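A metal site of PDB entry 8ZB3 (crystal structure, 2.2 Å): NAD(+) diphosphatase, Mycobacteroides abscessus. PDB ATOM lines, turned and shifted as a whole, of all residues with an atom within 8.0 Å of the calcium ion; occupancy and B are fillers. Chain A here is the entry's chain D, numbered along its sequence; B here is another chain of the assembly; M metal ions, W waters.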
ATOM      1  N   ALA A 191     -16.585  20.985 -14.812  1.00  0.00           N
ATOM      2  CA  ALA A 191     -16.925  20.787 -13.417  1.00  0.00           C
ATOM      3  C   ALA A 191     -18.297  20.130 -13.268  1.00  0.00           C
ATOM      4  O   ALA A 191     -19.165  20.315 -14.105  1.00  0.00           O
ATOM      5  CB  ALA A 191     -16.896  22.120 -12.728  1.00  0.00           C
ATOM      6  N   GLY A 192     -18.492  19.392 -12.182  1.00  0.00           N
ATOM      7  CA  GLY A 192     -19.821  18.908 -11.838  1.00  0.00           C
ATOM      8  C   GLY A 192     -19.886  18.302 -10.437  1.00  0.00           C
ATOM      9  O   GLY A 192     -18.878  17.941  -9.865  1.00  0.00           O
ATOM     10  N   PHE A 193     -21.096  18.201  -9.907  1.00  0.00           N
ATOM     11  CA  PHE A 193     -21.348  17.649  -8.592  1.00  0.00           C
ATOM     12  C   PHE A 193     -21.313  16.120  -8.651  1.00  0.00           C
ATOM     13  O   PHE A 193     -21.773  15.509  -9.603  1.00  0.00           O
ATOM     14  CB  PHE A 193     -22.667  18.207  -8.045  1.00  0.00           C
ATOM     15  CG  PHE A 193     -22.559  19.629  -7.536  1.00  0.00           C
ATOM     16  CD1 PHE A 193     -21.870  19.894  -6.354  1.00  0.00           C
ATOM     17  CD2 PHE A 193     -23.097  20.701  -8.248  1.00  0.00           C
ATOM     18  CE1 PHE A 193     -21.768  21.192  -5.867  1.00  0.00           C
ATOM     19  CE2 PHE A 193     -22.988  21.994  -7.766  1.00  0.00           C
ATOM     20  CZ  PHE A 193     -22.329  22.245  -6.587  1.00  0.00           C
ATOM     21  N   GLU A 195     -22.708  12.651  -7.820  1.00  0.00           N
ATOM     22  CA  GLU A 195     -24.027  12.110  -7.520  1.00  0.00           C
ATOM     23  C   GLU A 195     -23.920  10.911  -6.578  1.00  0.00           C
ATOM     24  O   GLU A 195     -22.884  10.298  -6.471  1.00  0.00           O
ATOM     25  CB  GLU A 195     -24.734  11.671  -8.800  1.00  0.00           C
ATOM     26  CG  GLU A 195     -25.057  12.814  -9.746  1.00  0.00           C
ATOM     27  CD  GLU A 195     -25.930  12.415 -10.935  1.00  0.00           C
ATOM     28  OE1 GLU A 195     -26.309  13.320 -11.686  1.00  0.00           O
ATOM     29  OE2 GLU A 195     -26.255  11.216 -11.116  1.00  0.00           O
ATOM     30  N   ARG A 206     -18.332  10.800 -16.354  1.00  0.00           N
ATOM     31  CA  ARG A 206     -19.715  11.116 -16.683  1.00  0.00           C
ATOM     32  C   ARG A 206     -19.833  12.598 -17.045  1.00  0.00           C
ATOM     33  O   ARG A 206     -20.412  12.932 -18.067  1.00  0.00           O
ATOM     34  CB  ARG A 206     -20.643  10.743 -15.525  1.00  0.00           C
ATOM     35  CG  ARG A 206     -22.109  11.081 -15.741  1.00  0.00           C
ATOM     36  CD  ARG A 206     -22.984  10.689 -14.557  1.00  0.00           C
ATOM     37  NE  ARG A 206     -22.617  11.330 -13.300  1.00  0.00           N
ATOM     38  CZ  ARG A 206     -22.674  12.646 -13.063  1.00  0.00           C
ATOM     39  NH1 ARG A 206     -23.149  13.471 -13.975  1.00  0.00           N
ATOM     40  NH2 ARG A 206     -22.232  13.143 -11.926  1.00  0.00           N
ATOM     41  N   GLU A 207     -19.279  13.476 -16.219  1.00  0.00           N
ATOM     42  CA  GLU A 207     -19.446  14.921 -16.378  1.00  0.00           C
ATOM     43  C   GLU A 207     -18.739  15.405 -17.640  1.00  0.00           C
ATOM     44  O   GLU A 207     -19.253  16.249 -18.351  1.00  0.00           O
ATOM     45  CB  GLU A 207     -18.947  15.677 -15.157  1.00  0.00           C
ATOM     46  CG  GLU A 207     -19.907  15.535 -13.957  1.00  0.00           C
ATOM     47  CD  GLU A 207     -21.194  16.339 -14.026  1.00  0.00           C
ATOM     48  OE1 GLU A 207     -22.048  16.144 -13.149  1.00  0.00           O
ATOM     49  OE2 GLU A 207     -21.304  17.189 -14.965  1.00  0.00           O
ATOM     50  N   VAL A 208     -17.550  14.899 -17.926  1.00  0.00           N
ATOM     51  CA  VAL A 208     -16.862  15.279 -19.154  1.00  0.00           C
ATOM     52  C   VAL A 208     -17.707  14.873 -20.374  1.00  0.00           C
ATOM     53  O   VAL A 208     -17.896  15.670 -21.285  1.00  0.00           O
ATOM     54  CB  VAL A 208     -15.453  14.680 -19.194  1.00  0.00           C
ATOM     55  CG1 VAL A 208     -14.827  14.823 -20.566  1.00  0.00           C
ATOM     56  CG2 VAL A 208     -14.575  15.316 -18.137  1.00  0.00           C
ATOM     57  N   ALA A 209     -18.251  13.646 -20.359  1.00  0.00           N
ATOM     58  CA  ALA A 209     -19.095  13.165 -21.443  1.00  0.00           C
ATOM     59  C   ALA A 209     -20.326  14.058 -21.596  1.00  0.00           C
ATOM     60  O   ALA A 209     -20.635  14.450 -22.728  1.00  0.00           O
ATOM     61  CB  ALA A 209     -19.483  11.719 -21.198  1.00  0.00           C
ATOM     62  N   GLU A 210     -21.001  14.388 -20.484  1.00  0.00           N
ATOM     63  CA  GLU A 210     -22.202  15.221 -20.498  1.00  0.00           C
ATOM     64  C   GLU A 210     -21.889  16.596 -21.081  1.00  0.00           C
ATOM     65  O   GLU A 210     -22.724  17.147 -21.796  1.00  0.00           O
ATOM     66  CB  GLU A 210     -22.730  15.422 -19.071  1.00  0.00           C
ATOM     67  CG  GLU A 210     -24.183  15.789 -18.877  1.00  0.00           C
ATOM     68  CD  GLU A 210     -24.627  15.776 -17.412  1.00  0.00           C
ATOM     69  OE1 GLU A 210     -24.890  14.659 -16.840  1.00  0.00           O
ATOM     70  OE2 GLU A 210     -24.692  16.880 -16.823  1.00  0.00           O
ATOM     71  N   GLU A 211     -20.726  17.175 -20.770  1.00  0.00           N
ATOM     72  CA  GLU A 211     -20.482  18.564 -21.092  1.00  0.00           C
ATOM     73  C   GLU A 211     -19.917  18.721 -22.511  1.00  0.00           C
ATOM     74  O   GLU A 211     -20.312  19.637 -23.237  1.00  0.00           O
ATOM     75  CB  GLU A 211     -19.515  19.209 -20.100  1.00  0.00           C
ATOM     76  CG  GLU A 211     -20.023  19.199 -18.675  1.00  0.00           C
ATOM     77  CD  GLU A 211     -21.159  20.181 -18.394  1.00  0.00           C
ATOM     78  OE1 GLU A 211     -22.253  19.731 -17.970  1.00  0.00           O
ATOM     79  OE2 GLU A 211     -20.947  21.394 -18.601  1.00  0.00           O
ATOM     80  N   ASP A 251     -26.618  17.688 -23.732  1.00  0.00           N
ATOM     81  CA  ASP A 251     -26.587  17.199 -22.359  1.00  0.00           C
ATOM     82  C   ASP A 251     -25.822  18.144 -21.438  1.00  0.00           C
ATOM     83  O   ASP A 251     -25.985  17.993 -20.232  1.00  0.00           O
ATOM     84  CB  ASP A 251     -26.050  15.765 -22.261  1.00  0.00           C
ATOM     85  CG  ASP A 251     -27.045  14.675 -22.635  1.00  0.00           C
ATOM     86  OD1 ASP A 251     -28.029  14.960 -23.340  1.00  0.00           O
ATOM     87  OD2 ASP A 251     -26.826  13.532 -22.174  1.00  0.00           O
ATOM     88  N   GLY A 252     -25.071  19.128 -21.968  1.00  0.00           N
ATOM     89  CA  GLY A 252     -24.203  19.971 -21.173  1.00  0.00           C
ATOM     90  C   GLY A 252     -24.649  21.438 -21.143  1.00  0.00           C
ATOM     91  O   GLY A 252     -25.621  21.815 -21.810  1.00  0.00           O
ATOM     92  N   GLU A 253     -23.899  22.279 -20.411  1.00  0.00           N
ATOM     93  CA  GLU A 253     -24.131  23.714 -20.407  1.00  0.00           C
ATOM     94  C   GLU A 253     -22.971  24.437 -21.099  1.00  0.00           C
ATOM     95  O   GLU A 253     -22.713  25.595 -20.819  1.00  0.00           O
ATOM     96  CB  GLU A 253     -24.264  24.304 -18.993  1.00  0.00           C
ATOM     97  CG  GLU A 253     -25.215  23.562 -18.062  1.00  0.00           C
ATOM     98  CD  GLU A 253     -24.510  22.732 -16.988  1.00  0.00           C
ATOM     99  OE1 GLU A 253     -23.611  23.285 -16.324  1.00  0.00           O
ATOM    100  OE2 GLU A 253     -24.869  21.538 -16.808  1.00  0.00           O
ATOM    101  N   ILE A 254     -22.264  23.745 -21.999  1.00  0.00           N
ATOM    102  CA  ILE A 254     -21.120  24.300 -22.704  1.00  0.00           C
ATOM    103  C   ILE A 254     -21.573  24.787 -24.082  1.00  0.00           C
ATOM    104  O   ILE A 254     -22.229  24.065 -24.829  1.00  0.00           O
ATOM    105  CB  ILE A 254     -19.989  23.260 -22.815  1.00  0.00           C
ATOM    106  CG1 ILE A 254     -19.455  22.824 -21.441  1.00  0.00           C
ATOM    107  CG2 ILE A 254     -18.846  23.763 -23.703  1.00  0.00           C
ATOM    108  CD1 ILE A 254     -18.742  23.925 -20.662  1.00  0.00           C
ATOM    109  N   ASP B  20     -29.311  10.979 -17.576  1.00  0.00           N
ATOM    110  CA  ASP B  20     -29.616  12.209 -16.865  1.00  0.00           C
ATOM    111  C   ASP B  20     -30.681  12.993 -17.643  1.00  0.00           C
ATOM    112  O   ASP B  20     -31.610  13.538 -17.043  1.00  0.00           O
ATOM    113  CB  ASP B  20     -28.308  12.987 -16.666  1.00  0.00           C
ATOM    114  CG  ASP B  20     -28.455  14.442 -16.232  1.00  0.00           C
ATOM    115  OD1 ASP B  20     -28.955  14.679 -15.120  1.00  0.00           O
ATOM    116  OD2 ASP B  20     -28.038  15.316 -17.012  1.00  0.00           O
HETATM  117 CA    CA M   1     -23.237  18.693 -15.822  1.00  0.00          CA
HETATM  118  O   HOH W   1     -21.110  20.287 -15.194  1.00  0.00           O
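OE1 of Glu 210 lies within salt-bridge range of NH1 of Arg 206, at 3.6 Å. The backbone NH of Gly 252 is in hydrogen-bond range of the backbone carbonyl oxygen of Glu 210 (3.1 Å). The guanidinium group (NH1) of Arg 206 lies within salt-bridge range of the side-chain carboxylate (OE1) of Glu 207 (3.0 Å).
Residues that only touch the calcium ion: Glu 253 (3.4 Å). Within 4 Å of the calcium ion: Glu 207, Glu 210, Glu 211 and Glu 253. Along chain A the residues within 4 Å of the calcium ion span positions 207 to 253. The nearest printed residue that does not touch the calcium ion is Ala 191 (4.7 Å).
The calcium ion is bound by the side-chain carboxylate (OE2) of Glu 210 (2.5 Å), the side-chain carboxylate (OE1) of Glu 211 (2.6 Å), the side-chain carboxylate (OE2) of Glu 207 (2.6 Å) and water W1 (2.7 Å).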
